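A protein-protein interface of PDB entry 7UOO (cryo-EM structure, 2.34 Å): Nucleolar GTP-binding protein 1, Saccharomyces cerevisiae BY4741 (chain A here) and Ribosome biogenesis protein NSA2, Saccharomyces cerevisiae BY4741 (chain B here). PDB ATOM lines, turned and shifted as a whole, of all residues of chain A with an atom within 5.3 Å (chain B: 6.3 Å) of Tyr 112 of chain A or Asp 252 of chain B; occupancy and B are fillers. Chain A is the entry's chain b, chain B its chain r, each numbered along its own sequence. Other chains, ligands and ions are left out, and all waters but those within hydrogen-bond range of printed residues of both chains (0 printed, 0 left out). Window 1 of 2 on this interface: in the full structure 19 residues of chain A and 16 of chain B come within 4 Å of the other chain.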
ATOM      1  N   VAL A  50       7.699  14.832   4.973  1.00  0.00           N
ATOM      2  CA  VAL A  50       6.842  14.052   4.075  1.00  0.00           C
ATOM      3  C   VAL A  50       7.433  12.667   3.824  1.00  0.00           C
ATOM      4  O   VAL A  50       6.737  11.644   3.921  1.00  0.00           O
ATOM      5  CB  VAL A  50       6.617  14.815   2.757  1.00  0.00           C
ATOM      6  CG1 VAL A  50       5.998  13.903   1.706  1.00  0.00           C
ATOM      7  CG2 VAL A  50       5.745  16.033   2.993  1.00  0.00           C
ATOM      8  N   GLN A 107       2.920   6.939  -3.750  1.00  0.00           N
ATOM      9  CA  GLN A 107       2.684   7.918  -4.807  1.00  0.00           C
ATOM     10  C   GLN A 107       2.518   9.324  -4.241  1.00  0.00           C
ATOM     11  O   GLN A 107       3.058  10.292  -4.795  1.00  0.00           O
ATOM     12  CB  GLN A 107       1.459   7.523  -5.625  1.00  0.00           C
ATOM     13  CG  GLN A 107       1.328   8.308  -6.912  1.00  0.00           C
ATOM     14  CD  GLN A 107       2.601   8.268  -7.731  1.00  0.00           C
ATOM     15  OE1 GLN A 107       3.057   7.200  -8.139  1.00  0.00           O
ATOM     16  NE2 GLN A 107       3.193   9.433  -7.963  1.00  0.00           N
ATOM     17  N   VAL A 108       1.775   9.454  -3.137  1.00  0.00           N
ATOM     18  CA  VAL A 108       1.574  10.764  -2.522  1.00  0.00           C
ATOM     19  C   VAL A 108       2.904  11.343  -2.051  1.00  0.00           C
ATOM     20  O   VAL A 108       3.195  12.529  -2.272  1.00  0.00           O
ATOM     21  CB  VAL A 108       0.554  10.667  -1.372  1.00  0.00           C
ATOM     22  CG1 VAL A 108       0.536  11.952  -0.554  1.00  0.00           C
ATOM     23  CG2 VAL A 108      -0.828  10.372  -1.918  1.00  0.00           C
ATOM     24  N   ALA A 109       3.739  10.512  -1.418  1.00  0.00           N
ATOM     25  CA  ALA A 109       5.036  10.987  -0.940  1.00  0.00           C
ATOM     26  C   ALA A 109       5.905  11.490  -2.089  1.00  0.00           C
ATOM     27  O   ALA A 109       6.492  12.580  -2.007  1.00  0.00           O
ATOM     28  CB  ALA A 109       5.753   9.879  -0.172  1.00  0.00           C
ATOM     29  N   ARG A 110       5.987  10.718  -3.178  1.00  0.00           N
ATOM     30  CA  ARG A 110       6.821  11.136  -4.305  1.00  0.00           C
ATOM     31  C   ARG A 110       6.305  12.429  -4.931  1.00  0.00           C
ATOM     32  O   ARG A 110       7.084  13.362  -5.195  1.00  0.00           O
ATOM     33  CB  ARG A 110       6.897  10.022  -5.349  1.00  0.00           C
ATOM     34  CG  ARG A 110       7.750   8.836  -4.930  1.00  0.00           C
ATOM     35  CD  ARG A 110       8.053   7.936  -6.113  1.00  0.00           C
ATOM     36  NE  ARG A 110       6.836   7.462  -6.759  1.00  0.00           N
ATOM     37  CZ  ARG A 110       6.229   6.323  -6.460  1.00  0.00           C
ATOM     38  NH1 ARG A 110       6.705   5.508  -5.534  1.00  0.00           N
ATOM     39  NH2 ARG A 110       5.115   5.992  -7.107  1.00  0.00           N
ATOM     40  N   ASP A 111       4.986  12.514  -5.149  1.00  0.00           N
ATOM     41  CA  ASP A 111       4.407  13.702  -5.770  1.00  0.00           C
ATOM     42  C   ASP A 111       4.652  14.949  -4.930  1.00  0.00           C
ATOM     43  O   ASP A 111       5.002  16.008  -5.464  1.00  0.00           O
ATOM     44  CB  ASP A 111       2.907  13.509  -5.993  1.00  0.00           C
ATOM     45  CG  ASP A 111       2.600  12.423  -6.997  1.00  0.00           C
ATOM     46  OD1 ASP A 111       3.549  11.823  -7.543  1.00  0.00           O
ATOM     47  OD2 ASP A 111       1.404  12.166  -7.245  1.00  0.00           O
ATOM     48  N   TYR A 112       4.496  14.843  -3.611  1.00  0.00           N
ATOM     49  CA  TYR A 112       4.621  16.054  -2.813  1.00  0.00           C
ATOM     50  C   TYR A 112       6.068  16.434  -2.529  1.00  0.00           C
ATOM     51  O   TYR A 112       6.350  17.620  -2.346  1.00  0.00           O
ATOM     52  CB  TYR A 112       3.813  15.923  -1.528  1.00  0.00           C
ATOM     53  CG  TYR A 112       2.377  16.316  -1.758  1.00  0.00           C
ATOM     54  CD1 TYR A 112       1.976  17.639  -1.641  1.00  0.00           C
ATOM     55  CD2 TYR A 112       1.434  15.374  -2.142  1.00  0.00           C
ATOM     56  CE1 TYR A 112       0.669  18.009  -1.869  1.00  0.00           C
ATOM     57  CE2 TYR A 112       0.124  15.736  -2.373  1.00  0.00           C
ATOM     58  CZ  TYR A 112      -0.253  17.055  -2.235  1.00  0.00           C
ATOM     59  OH  TYR A 112      -1.556  17.419  -2.463  1.00  0.00           O
ATOM     60  N   VAL A 113       7.007  15.482  -2.532  1.00  0.00           N
ATOM     61  CA  VAL A 113       8.414  15.881  -2.500  1.00  0.00           C
ATOM     62  C   VAL A 113       8.783  16.629  -3.780  1.00  0.00           C
ATOM     63  O   VAL A 113       9.456  17.678  -3.744  1.00  0.00           O
ATOM     64  CB  VAL A 113       9.317  14.655  -2.269  1.00  0.00           C
ATOM     65  CG1 VAL A 113      10.777  15.011  -2.495  1.00  0.00           C
ATOM     66  CG2 VAL A 113       9.123  14.116  -0.865  1.00  0.00           C
ATOM     67  N   ARG A 114       8.318  16.124  -4.929  1.00  0.00           N
ATOM     68  CA  ARG A 114       8.573  16.822  -6.186  1.00  0.00           C
ATOM     69  C   ARG A 114       7.958  18.219  -6.181  1.00  0.00           C
ATOM     70  O   ARG A 114       8.571  19.173  -6.670  1.00  0.00           O
ATOM     71  CB  ARG A 114       8.040  16.009  -7.361  1.00  0.00           C
ATOM     72  CG  ARG A 114       8.487  16.531  -8.713  1.00  0.00           C
ATOM     73  CD  ARG A 114       7.853  15.767  -9.866  1.00  0.00           C
ATOM     74  NE  ARG A 114       8.015  14.325  -9.738  1.00  0.00           N
ATOM     75  CZ  ARG A 114       7.032  13.486  -9.440  1.00  0.00           C
ATOM     76  NH1 ARG A 114       5.793  13.910  -9.262  1.00  0.00           N
ATOM     77  NH2 ARG A 114       7.301  12.189  -9.316  1.00  0.00           N
ATOM     78  N   LEU A 115       6.747  18.358  -5.633  1.00  0.00           N
ATOM     79  CA  LEU A 115       6.126  19.679  -5.544  1.00  0.00           C
ATOM     80  C   LEU A 115       6.877  20.592  -4.582  1.00  0.00           C
ATOM     81  O   LEU A 115       6.994  21.797  -4.830  1.00  0.00           O
ATOM     82  CB  LEU A 115       4.666  19.554  -5.122  1.00  0.00           C
ATOM     83  CG  LEU A 115       3.699  19.139  -6.226  1.00  0.00           C
ATOM     84  CD1 LEU A 115       2.275  19.112  -5.699  1.00  0.00           C
ATOM     85  CD2 LEU A 115       3.825  20.072  -7.420  1.00  0.00           C
ATOM     86  N   LEU A 116       7.380  20.043  -3.474  1.00  0.00           N
ATOM     87  CA  LEU A 116       8.121  20.845  -2.510  1.00  0.00           C
ATOM     88  C   LEU A 116       9.458  21.313  -3.056  1.00  0.00           C
ATOM     89  O   LEU A 116      10.054  22.228  -2.482  1.00  0.00           O
ATOM     90  CB  LEU A 116       8.335  20.057  -1.220  1.00  0.00           C
ATOM     91  CG  LEU A 116       7.176  20.109  -0.228  1.00  0.00           C
ATOM     92  CD1 LEU A 116       7.299  19.006   0.802  1.00  0.00           C
ATOM     93  CD2 LEU A 116       7.140  21.468   0.440  1.00  0.00           C
ATOM     94  N   LYS A 117       9.943  20.701  -4.139  1.00  0.00           N
ATOM     95  CA  LYS A 117      11.128  21.242  -4.808  1.00  0.00           C
ATOM     96  C   LYS A 117      10.942  22.696  -5.251  1.00  0.00           C
ATOM     97  O   LYS A 117      11.928  23.433  -5.367  1.00  0.00           O
ATOM     98  CB  LYS A 117      11.499  20.384  -6.015  1.00  0.00           C
ATOM     99  CG  LYS A 117      12.441  19.239  -5.708  1.00  0.00           C
ATOM    100  CD  LYS A 117      12.332  18.146  -6.757  1.00  0.00           C
ATOM    101  CE  LYS A 117      12.511  18.695  -8.161  1.00  0.00           C
ATOM    102  NZ  LYS A 117      12.287  17.644  -9.189  1.00  0.00           N
ATOM    103  N   GLN A 127       2.044  24.360   3.883  1.00  0.00           N
ATOM    104  CA  GLN A 127       0.766  23.936   3.317  1.00  0.00           C
ATOM    105  C   GLN A 127       0.915  22.663   2.491  1.00  0.00           C
ATOM    106  O   GLN A 127       0.070  21.766   2.569  1.00  0.00           O
ATOM    107  CB  GLN A 127       0.164  25.055   2.468  1.00  0.00           C
ATOM    108  CG  GLN A 127      -0.385  26.220   3.267  1.00  0.00           C
ATOM    109  CD  GLN A 127      -1.408  25.790   4.295  1.00  0.00           C
ATOM    110  OE1 GLN A 127      -2.534  25.434   3.954  1.00  0.00           O
ATOM    111  NE2 GLN A 127      -1.019  25.820   5.564  1.00  0.00           N
ATOM    112  N   LEU A 128       1.985  22.565   1.697  1.00  0.00           N
ATOM    113  CA  LEU A 128       2.205  21.359   0.902  1.00  0.00           C
ATOM    114  C   LEU A 128       2.463  20.140   1.788  1.00  0.00           C
ATOM    115  O   LEU A 128       1.932  19.051   1.528  1.00  0.00           O
ATOM    116  CB  LEU A 128       3.362  21.575  -0.072  1.00  0.00           C
ATOM    117  CG  LEU A 128       3.115  22.535  -1.240  1.00  0.00           C
ATOM    118  CD1 LEU A 128       4.427  22.911  -1.905  1.00  0.00           C
ATOM    119  CD2 LEU A 128       2.163  21.923  -2.256  1.00  0.00           C
ATOM    120  N   ALA A 131      -0.762  19.099   3.356  1.00  0.00           N
ATOM    121  CA  ALA A 131      -1.596  18.442   2.356  1.00  0.00           C
ATOM    122  C   ALA A 131      -1.168  16.997   2.141  1.00  0.00           C
ATOM    123  O   ALA A 131      -2.015  16.098   2.063  1.00  0.00           O
ATOM    124  CB  ALA A 131      -1.550  19.218   1.041  1.00  0.00           C
ATOM    125  N   ALA A 132       0.142  16.753   2.060  1.00  0.00           N
ATOM    126  CA  ALA A 132       0.634  15.389   1.877  1.00  0.00           C
ATOM    127  C   ALA A 132       0.262  14.502   3.061  1.00  0.00           C
ATOM    128  O   ALA A 132      -0.225  13.376   2.885  1.00  0.00           O
ATOM    129  CB  ALA A 132       2.148  15.402   1.673  1.00  0.00           C
ATOM    130  N   ARG A 135      -3.528  13.781   3.029  1.00  0.00           N
ATOM    131  CA  ARG A 135      -3.902  12.789   2.022  1.00  0.00           C
ATOM    132  C   ARG A 135      -3.508  11.381   2.460  1.00  0.00           C
ATOM    133  O   ARG A 135      -4.287  10.427   2.293  1.00  0.00           O
ATOM    134  CB  ARG A 135      -3.270  13.148   0.676  1.00  0.00           C
ATOM    135  CG  ARG A 135      -3.935  14.342  -0.008  1.00  0.00           C
ATOM    136  CD  ARG A 135      -3.169  14.805  -1.236  1.00  0.00           C
ATOM    137  NE  ARG A 135      -3.262  13.869  -2.348  1.00  0.00           N
ATOM    138  CZ  ARG A 135      -3.852  14.133  -3.505  1.00  0.00           C
ATOM    139  NH1 ARG A 135      -4.411  15.306  -3.745  1.00  0.00           N
ATOM    140  NH2 ARG A 135      -3.874  13.198  -4.450  1.00  0.00           N
ATOM    141  N   ASN B 247      -9.657  26.964  -5.641  1.00  0.00           N
ATOM    142  CA  ASN B 247      -8.630  26.765  -4.624  1.00  0.00           C
ATOM    143  C   ASN B 247      -7.308  27.302  -5.158  1.00  0.00           C
ATOM    144  O   ASN B 247      -7.247  27.898  -6.237  1.00  0.00           O
ATOM    145  CB  ASN B 247      -8.536  25.288  -4.223  1.00  0.00           C
ATOM    146  CG  ASN B 247      -7.848  24.435  -5.273  1.00  0.00           C
ATOM    147  OD1 ASN B 247      -8.032  24.632  -6.472  1.00  0.00           O
ATOM    148  ND2 ASN B 247      -7.047  23.480  -4.822  1.00  0.00           N
ATOM    149  N   GLU B 248      -6.240  27.094  -4.387  1.00  0.00           N
ATOM    150  CA  GLU B 248      -4.888  27.436  -4.819  1.00  0.00           C
ATOM    151  C   GLU B 248      -4.093  26.154  -5.033  1.00  0.00           C
ATOM    152  O   GLU B 248      -3.610  25.544  -4.059  1.00  0.00           O
ATOM    153  CB  GLU B 248      -4.189  28.342  -3.800  1.00  0.00           C
ATOM    154  CG  GLU B 248      -4.786  29.744  -3.672  1.00  0.00           C
ATOM    155  CD  GLU B 248      -4.471  30.660  -4.853  1.00  0.00           C
ATOM    156  OE1 GLU B 248      -3.744  30.242  -5.779  1.00  0.00           O
ATOM    157  OE2 GLU B 248      -4.953  31.813  -4.854  1.00  0.00           O
ATOM    158  N   PRO B 249      -3.955  25.691  -6.279  1.00  0.00           N
ATOM    159  CA  PRO B 249      -3.163  24.480  -6.531  1.00  0.00           C
ATOM    160  C   PRO B 249      -1.700  24.623  -6.161  1.00  0.00           C
ATOM    161  O   PRO B 249      -1.068  23.619  -5.822  1.00  0.00           O
ATOM    162  CB  PRO B 249      -3.354  24.238  -8.037  1.00  0.00           C
ATOM    163  CG  PRO B 249      -3.867  25.519  -8.588  1.00  0.00           C
ATOM    164  CD  PRO B 249      -4.625  26.185  -7.493  1.00  0.00           C
ATOM    165  N   ASP B 250      -1.146  25.839  -6.191  1.00  0.00           N
ATOM    166  CA  ASP B 250       0.217  26.037  -5.711  1.00  0.00           C
ATOM    167  C   ASP B 250       0.344  25.723  -4.226  1.00  0.00           C
ATOM    168  O   ASP B 250       1.414  25.309  -3.768  1.00  0.00           O
ATOM    169  CB  ASP B 250       0.678  27.468  -5.989  1.00  0.00           C
ATOM    170  CG  ASP B 250      -0.224  28.505  -5.352  1.00  0.00           C
ATOM    171  OD1 ASP B 250      -1.421  28.553  -5.704  1.00  0.00           O
ATOM    172  OD2 ASP B 250       0.260  29.267  -4.491  1.00  0.00           O
ATOM    173  N   ARG B 251      -0.732  25.906  -3.462  1.00  0.00           N
ATOM    174  CA  ARG B 251      -0.711  25.637  -2.031  1.00  0.00           C
ATOM    175  C   ARG B 251      -1.036  24.184  -1.704  1.00  0.00           C
ATOM    176  O   ARG B 251      -0.342  23.567  -0.892  1.00  0.00           O
ATOM    177  CB  ARG B 251      -1.693  26.556  -1.302  1.00  0.00           C
ATOM    178  CG  ARG B 251      -1.310  28.018  -1.302  1.00  0.00           C
ATOM    179  CD  ARG B 251      -2.356  28.828  -0.561  1.00  0.00           C
ATOM    180  NE  ARG B 251      -2.178  30.262  -0.740  1.00  0.00           N
ATOM    181  CZ  ARG B 251      -3.011  31.180  -0.271  1.00  0.00           C
ATOM    182  NH1 ARG B 251      -4.088  30.846   0.419  1.00  0.00           N
ATOM    183  NH2 ARG B 251      -2.759  32.464  -0.504  1.00  0.00           N
ATOM    184  N   ASP B 252      -2.083  23.620  -2.309  1.00  0.00           N
ATOM    185  CA  ASP B 252      -2.544  22.299  -1.892  1.00  0.00           C
ATOM    186  C   ASP B 252      -2.276  21.192  -2.908  1.00  0.00           C
ATOM    187  O   ASP B 252      -2.739  20.066  -2.708  1.00  0.00           O
ATOM    188  CB  ASP B 252      -4.031  22.338  -1.538  1.00  0.00           C
ATOM    189  CG  ASP B 252      -4.895  22.744  -2.699  1.00  0.00           C
ATOM    190  OD1 ASP B 252      -4.335  23.069  -3.764  1.00  0.00           O
ATOM    191  OD2 ASP B 252      -6.134  22.730  -2.550  1.00  0.00           O
ATOM    192  N   GLY B 253      -1.540  21.468  -3.981  1.00  0.00           N
ATOM    193  CA  GLY B 253      -1.103  20.409  -4.869  1.00  0.00           C
ATOM    194  C   GLY B 253      -2.159  19.790  -5.755  1.00  0.00           C
ATOM    195  O   GLY B 253      -1.892  18.754  -6.367  1.00  0.00           O
ATOM    196  N   CYS B 254      -3.350  20.380  -5.846  1.00  0.00           N
ATOM    197  CA  CYS B 254      -4.397  19.848  -6.707  1.00  0.00           C
ATOM    198  C   CYS B 254      -5.311  20.982  -7.144  1.00  0.00           C
ATOM    199  O   CYS B 254      -5.339  22.052  -6.533  1.00  0.00           O
ATOM    200  CB  CYS B 254      -5.209  18.750  -6.006  1.00  0.00           C
ATOM    201  SG  CYS B 254      -6.164  19.305  -4.577  1.00  0.00           S
ATOM    202  N   VAL B 255      -6.073  20.731  -8.205  1.00  0.00           N
ATOM    203  CA  VAL B 255      -6.975  21.720  -8.783  1.00  0.00           C
ATOM    204  C   VAL B 255      -8.407  21.303  -8.469  1.00  0.00           C
ATOM    205  O   VAL B 255      -8.842  20.210  -8.850  1.00  0.00           O
ATOM    206  CB  VAL B 255      -6.762  21.871 -10.297  1.00  0.00           C
ATOM    207  CG1 VAL B 255      -7.647  22.975 -10.851  1.00  0.00           C
ATOM    208  CG2 VAL B 255      -5.298  22.147 -10.607  1.00  0.00           C
ATOM    209  N   ASN B 256      -9.130  22.172  -7.768  1.00  0.00           N
ATOM    210  CA  ASN B 256     -10.545  21.995  -7.482  1.00  0.00           C
ATOM    211  C   ASN B 256     -11.336  23.077  -8.199  1.00  0.00           C
ATOM    212  O   ASN B 256     -10.944  24.246  -8.196  1.00  0.00           O
ATOM    213  CB  ASN B 256     -10.821  22.065  -5.978  1.00  0.00           C
ATOM    214  CG  ASN B 256     -10.094  20.994  -5.202  1.00  0.00           C
ATOM    215  OD1 ASN B 256      -9.961  19.862  -5.657  1.00  0.00           O
ATOM    216  ND2 ASN B 256      -9.619  21.347  -4.015  1.00  0.00           N
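OH of Tyr 112 of chain A lies within hydrogen-bond range of O of Asp 252 of chain B (2.9 Å).
Of chain B, only Asp 252 and Gly 253 come within 4 Å of Tyr 112 of chain A. Printed residues of chain B within 4 Å of Leu 115 of chain A: Gly 253. Of the printed residues of chain B, Gln 127 of chain A touches Arg 251 (3.7 Å). Printed residues of chain A within 4 Å of Arg 251 of chain B: Gln 127 (3.7 Å) and Leu 128 (3.3 Å). Asp 252 of chain B touches just one residue of chain A: Tyr 112 (2.9 Å). Printed residues of chain A within 4 Å of Gly 253 of chain B: Tyr 112 and Leu 115. The nearest residue of chain B that does not touch Tyr 112 of chain A is Cys 254 of chain B (4.8 Å). The nearest printed residue of chain A that does not touch Gly 253 of chain B is Leu 128 of chain A (4.1 Å).
The side-chain carboxylate (OD2) of Asp 252 of chain B is in hydrogen-bond range of the side-chain amide nitrogen (ND2) of Asn 247 of chain B (2.6 Å). O of Glu 248 of chain B lies close to OD1 of Asp 252 of chain B (2.6 Å).
Along chain A the printed residues that touch a printed residue of chain B span positions 112 to 128. Among the printed residues, no Asp or Glu carboxylate lies within 4 Å of a Lys or Arg side-chain nitrogen of the other chain.
Tyr 112 of chain A touches Gly 253 of chain B (OH to CA, 3.9 Å). CD1 of Leu 115 of chain A touches CA of Gly 253 of chain B, 3.7 Å away. CB of Gln 127 of chain A touches O of Arg 251 of chain B (3.7 Å). Asp 250 of chain B touches Leu 128 of chain A. CD2 of Leu 128 of chain A touches O of Arg 251 of chain B (3.3 Å).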
